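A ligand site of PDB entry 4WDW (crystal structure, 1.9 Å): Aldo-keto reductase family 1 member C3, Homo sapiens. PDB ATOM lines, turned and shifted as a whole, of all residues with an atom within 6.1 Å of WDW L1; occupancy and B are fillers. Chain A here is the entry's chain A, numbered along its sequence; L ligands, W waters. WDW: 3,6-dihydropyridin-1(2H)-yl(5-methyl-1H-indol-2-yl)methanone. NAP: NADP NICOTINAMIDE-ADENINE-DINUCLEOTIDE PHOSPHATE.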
ATOM      1  N   TYR A  24      12.050 -16.522 -13.542  1.00  0.00           N
ATOM      2  CA  TYR A  24      11.752 -16.245 -12.131  1.00  0.00           C
ATOM      3  C   TYR A  24      10.668 -15.151 -11.934  1.00  0.00           C
ATOM      4  O   TYR A  24      10.771 -14.095 -12.555  1.00  0.00           O
ATOM      5  CB  TYR A  24      13.003 -15.803 -11.367  1.00  0.00           C
ATOM      6  CG  TYR A  24      12.662 -15.548  -9.908  1.00  0.00           C
ATOM      7  CD1 TYR A  24      12.388 -16.620  -9.054  1.00  0.00           C
ATOM      8  CD2 TYR A  24      12.567 -14.250  -9.405  1.00  0.00           C
ATOM      9  CE1 TYR A  24      12.081 -16.441  -7.708  1.00  0.00           C
ATOM     10  CE2 TYR A  24      12.246 -14.037  -8.060  1.00  0.00           C
ATOM     11  CZ  TYR A  24      11.986 -15.152  -7.247  1.00  0.00           C
ATOM     12  OH  TYR A  24      11.682 -14.984  -5.919  1.00  0.00           O
ATOM     13  N   ALA A  52      15.517 -22.963 -12.733  1.00  0.00           N
ATOM     14  CA  ALA A  52      16.386 -23.379 -11.566  1.00  0.00           C
ATOM     15  C   ALA A  52      15.449 -24.106 -10.508  1.00  0.00           C
ATOM     16  O   ALA A  52      14.241 -23.771 -10.406  1.00  0.00           O
ATOM     17  CB  ALA A  52      16.990 -22.174 -10.876  1.00  0.00           C
ATOM     18  N   LEU A  54      15.587 -23.557  -7.554  1.00  0.00           N
ATOM     19  CA  LEU A  54      15.209 -22.494  -6.589  1.00  0.00           C
ATOM     20  C   LEU A  54      13.896 -21.780  -6.882  1.00  0.00           C
ATOM     21  O   LEU A  54      13.179 -21.326  -5.934  1.00  0.00           O
ATOM     22  CB  LEU A  54      16.297 -21.423  -6.512  1.00  0.00           C
ATOM     23  CG  LEU A  54      16.147 -20.165  -5.659  1.00  0.00           C
ATOM     24  CD1 LEU A  54      15.989 -20.551  -4.179  1.00  0.00           C
ATOM     25  CD2 LEU A  54      17.277 -19.197  -5.855  1.00  0.00           C
ATOM     26  N   TYR A  55      13.565 -21.647  -8.168  1.00  0.00           N
ATOM     27  CA  TYR A  55      12.501 -20.749  -8.623  1.00  0.00           C
ATOM     28  C   TYR A  55      11.141 -21.376  -8.366  1.00  0.00           C
ATOM     29  O   TYR A  55      10.144 -20.678  -8.562  1.00  0.00           O
ATOM     30  CB  TYR A  55      12.633 -20.471 -10.144  1.00  0.00           C
ATOM     31  CG  TYR A  55      13.910 -19.791 -10.524  1.00  0.00           C
ATOM     32  CD1 TYR A  55      14.300 -19.692 -11.868  1.00  0.00           C
ATOM     33  CD2 TYR A  55      14.755 -19.243  -9.553  1.00  0.00           C
ATOM     34  CE1 TYR A  55      15.480 -19.032 -12.194  1.00  0.00           C
ATOM     35  CE2 TYR A  55      15.944 -18.583  -9.894  1.00  0.00           C
ATOM     36  CZ  TYR A  55      16.271 -18.482 -11.218  1.00  0.00           C
ATOM     37  OH  TYR A  55      17.451 -17.879 -11.553  1.00  0.00           O
ATOM     38  N   LYS A  84      19.291 -25.295 -12.778  1.00  0.00           N
ATOM     39  CA  LYS A  84      20.481 -25.062 -11.923  1.00  0.00           C
ATOM     40  C   LYS A  84      20.407 -25.818 -10.594  1.00  0.00           C
ATOM     41  O   LYS A  84      19.306 -25.979  -9.997  1.00  0.00           O
ATOM     42  CB  LYS A  84      20.691 -23.568 -11.627  1.00  0.00           C
ATOM     43  CG  LYS A  84      20.419 -22.531 -12.752  1.00  0.00           C
ATOM     44  CD  LYS A  84      20.578 -21.105 -12.194  1.00  0.00           C
ATOM     45  CE  LYS A  84      20.239 -20.021 -13.237  1.00  0.00           C
ATOM     46  NZ  LYS A  84      18.777 -19.849 -13.530  1.00  0.00           N
ATOM     47  N   TRP A  86      20.922 -26.287  -6.750  1.00  0.00           N
ATOM     48  CA  TRP A  86      20.794 -25.363  -5.653  1.00  0.00           C
ATOM     49  C   TRP A  86      21.892 -25.683  -4.657  1.00  0.00           C
ATOM     50  O   TRP A  86      22.518 -26.750  -4.760  1.00  0.00           O
ATOM     51  CB  TRP A  86      19.383 -25.333  -4.998  1.00  0.00           C
ATOM     52  CG  TRP A  86      19.348 -24.306  -3.836  1.00  0.00           C
ATOM     53  CD1 TRP A  86      19.059 -24.581  -2.514  1.00  0.00           C
ATOM     54  CD2 TRP A  86      19.664 -22.900  -3.895  1.00  0.00           C
ATOM     55  NE1 TRP A  86      19.134 -23.421  -1.773  1.00  0.00           N
ATOM     56  CE2 TRP A  86      19.543 -22.383  -2.580  1.00  0.00           C
ATOM     57  CE3 TRP A  86      20.103 -22.029  -4.924  1.00  0.00           C
ATOM     58  CZ2 TRP A  86      19.785 -21.043  -2.262  1.00  0.00           C
ATOM     59  CZ3 TRP A  86      20.369 -20.701  -4.632  1.00  0.00           C
ATOM     60  CH2 TRP A  86      20.204 -20.204  -3.291  1.00  0.00           C
ATOM     61  N   SER A  87      22.198 -24.723  -3.778  1.00  0.00           N
ATOM     62  CA  SER A  87      23.433 -24.775  -2.979  1.00  0.00           C
ATOM     63  C   SER A  87      23.420 -25.849  -1.837  1.00  0.00           C
ATOM     64  O   SER A  87      24.466 -26.147  -1.275  1.00  0.00           O
ATOM     65  CB  SER A  87      23.770 -23.389  -2.438  1.00  0.00           C
ATOM     66  OG  SER A  87      24.234 -22.505  -3.491  1.00  0.00           O
ATOM     67  N   HIS A 117      24.419 -23.178  -9.191  1.00  0.00           N
ATOM     68  CA  HIS A 117      23.729 -21.875  -9.100  1.00  0.00           C
ATOM     69  C   HIS A 117      24.605 -20.809  -8.416  1.00  0.00           C
ATOM     70  O   HIS A 117      24.650 -19.625  -8.828  1.00  0.00           O
ATOM     71  CB  HIS A 117      22.407 -22.067  -8.312  1.00  0.00           C
ATOM     72  CG  HIS A 117      21.386 -21.018  -8.539  1.00  0.00           C
ATOM     73  ND1 HIS A 117      20.027 -21.286  -8.496  1.00  0.00           N
ATOM     74  CD2 HIS A 117      21.501 -19.696  -8.859  1.00  0.00           C
ATOM     75  CE1 HIS A 117      19.359 -20.169  -8.696  1.00  0.00           C
ATOM     76  NE2 HIS A 117      20.223 -19.196  -8.963  1.00  0.00           N
ATOM     77  N   SER A 118      25.360 -21.238  -7.401  1.00  0.00           N
ATOM     78  CA  SER A 118      26.190 -20.271  -6.688  1.00  0.00           C
ATOM     79  C   SER A 118      27.381 -21.000  -6.081  1.00  0.00           C
ATOM     80  O   SER A 118      27.288 -22.228  -5.834  1.00  0.00           O
ATOM     81  CB  SER A 118      25.346 -19.510  -5.646  1.00  0.00           C
ATOM     82  OG  SER A 118      26.045 -19.177  -4.468  1.00  0.00           O
ATOM     83  N   MET A 120      28.449 -20.851  -3.241  1.00  0.00           N
ATOM     84  CA  MET A 120      28.199 -21.119  -1.797  1.00  0.00           C
ATOM     85  C   MET A 120      27.597 -22.483  -1.557  1.00  0.00           C
ATOM     86  O   MET A 120      26.766 -22.957  -2.371  1.00  0.00           O
ATOM     87  CB  MET A 120      27.355 -20.033  -1.166  1.00  0.00           C
ATOM     88  CG  MET A 120      25.870 -20.103  -1.483  1.00  0.00           C
ATOM     89  SD  MET A 120      24.944 -18.995  -0.387  1.00  0.00           S
ATOM     90  CE  MET A 120      25.830 -17.429  -0.646  1.00  0.00           C
ATOM     91  N   ASN A 167      27.374 -16.961 -10.991  1.00  0.00           N
ATOM     92  CA  ASN A 167      27.822 -16.138  -9.816  1.00  0.00           C
ATOM     93  C   ASN A 167      29.263 -16.426  -9.416  1.00  0.00           C
ATOM     94  O   ASN A 167      29.632 -16.195  -8.279  1.00  0.00           O
ATOM     95  CB  ASN A 167      26.872 -16.349  -8.616  1.00  0.00           C
ATOM     96  CG  ASN A 167      25.492 -15.767  -8.917  1.00  0.00           C
ATOM     97  OD1 ASN A 167      25.375 -14.568  -9.117  1.00  0.00           O
ATOM     98  ND2 ASN A 167      24.468 -16.611  -8.944  1.00  0.00           N
ATOM     99  N   TYR A 216      22.376 -11.748 -16.264  1.00  0.00           N
ATOM    100  CA  TYR A 216      21.062 -11.722 -15.628  1.00  0.00           C
ATOM    101  C   TYR A 216      20.913 -10.354 -15.034  1.00  0.00           C
ATOM    102  O   TYR A 216      21.912  -9.639 -14.883  1.00  0.00           O
ATOM    103  CB  TYR A 216      20.900 -12.876 -14.593  1.00  0.00           C
ATOM    104  CG  TYR A 216      21.620 -12.790 -13.300  1.00  0.00           C
ATOM    105  CD1 TYR A 216      22.603 -13.706 -13.010  1.00  0.00           C
ATOM    106  CD2 TYR A 216      21.341 -11.759 -12.347  1.00  0.00           C
ATOM    107  CE1 TYR A 216      23.253 -13.683 -11.826  1.00  0.00           C
ATOM    108  CE2 TYR A 216      22.013 -11.705 -11.141  1.00  0.00           C
ATOM    109  CZ  TYR A 216      22.946 -12.690 -10.886  1.00  0.00           C
ATOM    110  OH  TYR A 216      23.641 -12.754  -9.718  1.00  0.00           O
ATOM    111  N   SER A 217      19.678 -10.009 -14.681  1.00  0.00           N
ATOM    112  CA  SER A 217      19.321  -8.646 -14.300  1.00  0.00           C
ATOM    113  C   SER A 217      19.807  -7.604 -15.353  1.00  0.00           C
ATOM    114  O   SER A 217      20.247  -6.502 -14.969  1.00  0.00           O
ATOM    115  CB  SER A 217      19.830  -8.336 -12.888  1.00  0.00           C
ATOM    116  OG  SER A 217      19.104  -9.074 -11.947  1.00  0.00           O
ATOM    117  N   GLN A 222      14.291  -6.946 -11.003  1.00  0.00           N
ATOM    118  CA  GLN A 222      12.855  -6.694 -10.785  1.00  0.00           C
ATOM    119  C   GLN A 222      12.710  -5.835  -9.542  1.00  0.00           C
ATOM    120  O   GLN A 222      11.610  -5.549  -9.144  1.00  0.00           O
ATOM    121  CB  GLN A 222      12.082  -8.011 -10.574  1.00  0.00           C
ATOM    122  CG  GLN A 222      12.536  -9.128 -11.533  1.00  0.00           C
ATOM    123  CD  GLN A 222      11.715 -10.391 -11.371  1.00  0.00           C
ATOM    124  OE1 GLN A 222      10.581 -10.333 -10.913  1.00  0.00           O
ATOM    125  NE2 GLN A 222      12.290 -11.571 -11.761  1.00  0.00           N
ATOM    126  N   PHE A 306      21.533  -7.218  -6.994  1.00  0.00           N
ATOM    127  CA  PHE A 306      21.163  -8.427  -6.285  1.00  0.00           C
ATOM    128  C   PHE A 306      22.038  -8.737  -5.048  1.00  0.00           C
ATOM    129  O   PHE A 306      23.153  -8.233  -4.897  1.00  0.00           O
ATOM    130  CB  PHE A 306      21.034  -9.653  -7.237  1.00  0.00           C
ATOM    131  CG  PHE A 306      20.701 -10.925  -6.526  1.00  0.00           C
ATOM    132  CD1 PHE A 306      19.452 -11.095  -5.938  1.00  0.00           C
ATOM    133  CD2 PHE A 306      21.657 -11.933  -6.375  1.00  0.00           C
ATOM    134  CE1 PHE A 306      19.148 -12.251  -5.218  1.00  0.00           C
ATOM    135  CE2 PHE A 306      21.360 -13.084  -5.678  1.00  0.00           C
ATOM    136  CZ  PHE A 306      20.108 -13.249  -5.098  1.00  0.00           C
HETATM  137  C14 WDW L   1      22.933 -16.696  -4.598  1.00  0.00           C
HETATM  138  C10 WDW L   1      22.505 -16.570  -5.906  1.00  0.00           C
HETATM  139  C12 WDW L   1      20.703 -16.468  -3.714  1.00  0.00           C
HETATM  140  C11 WDW L   1      18.938 -16.128  -5.592  1.00  0.00           C
HETATM  141  C8  WDW L   1      20.227 -16.328  -5.012  1.00  0.00           C
HETATM  142  C15 WDW L   1      22.061 -16.644  -3.545  1.00  0.00           C
HETATM  143  C7  WDW L   1      21.144 -16.383  -6.056  1.00  0.00           C
HETATM  144  C13 WDW L   1      19.086 -16.052  -6.971  1.00  0.00           C
HETATM  145  C4  WDW L   1      16.278 -12.495  -8.840  1.00  0.00           C
HETATM  146  C5  WDW L   1      16.755 -12.729  -7.607  1.00  0.00           C
HETATM  147  C16 WDW L   1      18.188 -15.901  -8.077  1.00  0.00           C
HETATM  148  C3  WDW L   1      15.801 -13.597  -9.748  1.00  0.00           C
HETATM  149  C6  WDW L   1      16.852 -14.097  -6.997  1.00  0.00           C
HETATM  150  C2  WDW L   1      16.273 -14.985  -9.286  1.00  0.00           C
HETATM  151  C17 WDW L   1      22.619 -16.785  -2.165  1.00  0.00           C
HETATM  152  N9  WDW L   1      20.418 -16.209  -7.199  1.00  0.00           N
HETATM  153  N1  WDW L   1      17.118 -15.038  -8.073  1.00  0.00           N
HETATM  154  O18 WDW L   1      18.431 -16.627  -9.036  1.00  0.00           O
HETATM  155  PA  NAP L   2      15.462  -8.624 -15.680  1.00  0.00           P
HETATM  156  O1A NAP L   2      16.579  -7.654 -15.325  1.00  0.00           O
HETATM  157  O2A NAP L   2      15.513  -9.494 -16.937  1.00  0.00           O
HETATM  158  O5B NAP L   2      14.012  -7.899 -15.724  1.00  0.00           O
HETATM  159  C5B NAP L   2      13.705  -6.762 -14.869  1.00  0.00           C
HETATM  160  C4B NAP L   2      12.323  -6.215 -15.248  1.00  0.00           C
HETATM  161  O4B NAP L   2      12.333  -5.674 -16.572  1.00  0.00           O
HETATM  162  C3B NAP L   2      11.302  -7.290 -15.324  1.00  0.00           C
HETATM  163  O3B NAP L   2      10.769  -7.395 -14.046  1.00  0.00           O
HETATM  164  C2B NAP L   2      10.293  -6.826 -16.373  1.00  0.00           C
HETATM  165  O2B NAP L   2       9.044  -6.579 -15.714  1.00  0.00           O
HETATM  166  C1B NAP L   2      10.951  -5.588 -16.975  1.00  0.00           C
HETATM  167  N9A NAP L   2      10.968  -5.522 -18.427  1.00  0.00           N
HETATM  168  C8A NAP L   2      11.235  -6.562 -19.299  1.00  0.00           C
HETATM  169  N7A NAP L   2      11.197  -6.134 -20.553  1.00  0.00           N
HETATM  170  C5A NAP L   2      10.883  -4.779 -20.511  1.00  0.00           C
HETATM  171  C6A NAP L   2      10.689  -3.803 -21.504  1.00  0.00           C
HETATM  172  N6A NAP L   2      10.783  -4.102 -22.878  1.00  0.00           N
HETATM  173  N1A NAP L   2      10.388  -2.528 -21.131  1.00  0.00           N
HETATM  174  C2A NAP L   2      10.271  -2.290 -19.809  1.00  0.00           C
HETATM  175  N3A NAP L   2      10.434  -3.152 -18.778  1.00  0.00           N
HETATM  176  C4A NAP L   2      10.750  -4.392 -19.195  1.00  0.00           C
HETATM  177  O3  NAP L   2      15.094  -9.487 -14.383  1.00  0.00           O
HETATM  178  PN  NAP L   2      15.786 -10.618 -13.497  1.00  0.00           P
HETATM  179  O1N NAP L   2      16.708  -9.909 -12.518  1.00  0.00           O
HETATM  180  O2N NAP L   2      14.689 -11.469 -12.936  1.00  0.00           O
HETATM  181  O5D NAP L   2      16.800 -11.376 -14.565  1.00  0.00           O
HETATM  182  C5D NAP L   2      16.323 -12.286 -15.590  1.00  0.00           C
HETATM  183  C4D NAP L   2      16.446 -13.749 -15.291  1.00  0.00           C
HETATM  184  O4D NAP L   2      17.767 -14.063 -14.916  1.00  0.00           O
HETATM  185  C3D NAP L   2      15.624 -14.230 -14.128  1.00  0.00           C
HETATM  186  O3D NAP L   2      14.203 -14.272 -14.436  1.00  0.00           O
HETATM  187  C2D NAP L   2      16.320 -15.541 -13.868  1.00  0.00           C
HETATM  188  O2D NAP L   2      15.890 -16.391 -14.956  1.00  0.00           O
HETATM  189  C1D NAP L   2      17.805 -15.186 -14.066  1.00  0.00           C
HETATM  190  N1N NAP L   2      18.575 -14.832 -12.827  1.00  0.00           N
HETATM  191  C2N NAP L   2      19.550 -15.656 -12.435  1.00  0.00           C
HETATM  192  C3N NAP L   2      20.264 -15.342 -11.296  1.00  0.00           C
HETATM  193  C7N NAP L   2      21.353 -16.224 -10.852  1.00  0.00           C
HETATM  194  O7N NAP L   2      21.736 -16.186  -9.698  1.00  0.00           O
HETATM  195  N7N NAP L   2      21.845 -17.085 -11.796  1.00  0.00           N
HETATM  196  C4N NAP L   2      19.954 -14.221 -10.567  1.00  0.00           C
HETATM  197  C5N NAP L   2      18.948 -13.377 -10.986  1.00  0.00           C
HETATM  198  C6N NAP L   2      18.266 -13.720 -12.140  1.00  0.00           C
HETATM  199  P2B NAP L   2       7.691  -7.260 -16.381  1.00  0.00           P
HETATM  200  O1X NAP L   2       7.764  -8.662 -15.844  1.00  0.00           O
HETATM  201  O2X NAP L   2       6.614  -6.513 -15.646  1.00  0.00           O
HETATM  202  O3X NAP L   2       7.747  -7.026 -17.858  1.00  0.00           O
HETATM  203  O   HOH W   1      15.597  -9.572 -10.223  1.00  0.00           O
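Water W1 lies within hydrogen-bond range of O1N of NAP L2 (2.6 Å) and N of Gln 222 (3.0 Å).
N9 of WDW L1 lies within hydrogen-bond range of O7N of NAP L2 (2.8 Å).
The backbone NH (N) of Ser 217 is in hydrogen-bond range of an oxygen (O5D) of NAP L2 (3.2 Å).
OG of Ser 217 lies within hydrogen-bond range of O1N of NAP L2, at 2.6 Å.
The backbone NH (N) of Tyr 24 sits at hydrogen-bond distance from an oxygen (O3D) of NAP L2 (3.2 Å).
NE2 of His 117 sits at hydrogen-bond distance from O18 of WDW L1, at 3.1 Å.
The side-chain amide nitrogen of Gln 222 is in hydrogen-bond range of an oxygen (O2N) of NAP L2 (2.7 Å).
ND2 of Asn 167 lies within hydrogen-bond range of O7N of NAP L2.
The side-chain hydroxyl of Tyr 55 lies within hydrogen-bond range of an oxygen (O18) of WDW L1, 3.0 Å away.
O7N of NAP L2 is in hydrogen-bond range of NE2 of His 117 (3.4 Å).
Residues that only touch WDW L1: Tyr 24 (3.3 Å), Leu 54 (3.5 Å), Trp 86 (3.8 Å), Ser 118 (3.9 Å), Met 120 (3.6 Å), Asn 167 (3.6 Å) and Phe 306 (3.1 Å).
Nine residues have an atom within 4 Å of WDW L1: Tyr 24, Leu 54, Tyr 55, Trp 86, His 117, Ser 118, Met 120, Asn 167 and Phe 306.
The backbone carbonyl oxygen of Met 120 is in hydrogen-bond range of the side-chain hydroxyl of Ser 87 (2.8 Å).
NZ of Lys 84 lies within hydrogen-bond range of OH of Tyr 55.
O of His 117 lies within hydrogen-bond range of ND2 of Asn 167.
The backbone NH (N) of Met 120 lies close to the side-chain hydroxyl (OG) of Ser 118, 3.2 Å away.
O of Tyr 24 lies within hydrogen-bond range of NE2 of Gln 222.
The side-chain hydroxyl (OH) of Tyr 216 is in hydrogen-bond range of the side-chain amide oxygen (OD1) of Asn 167 (2.6 Å).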
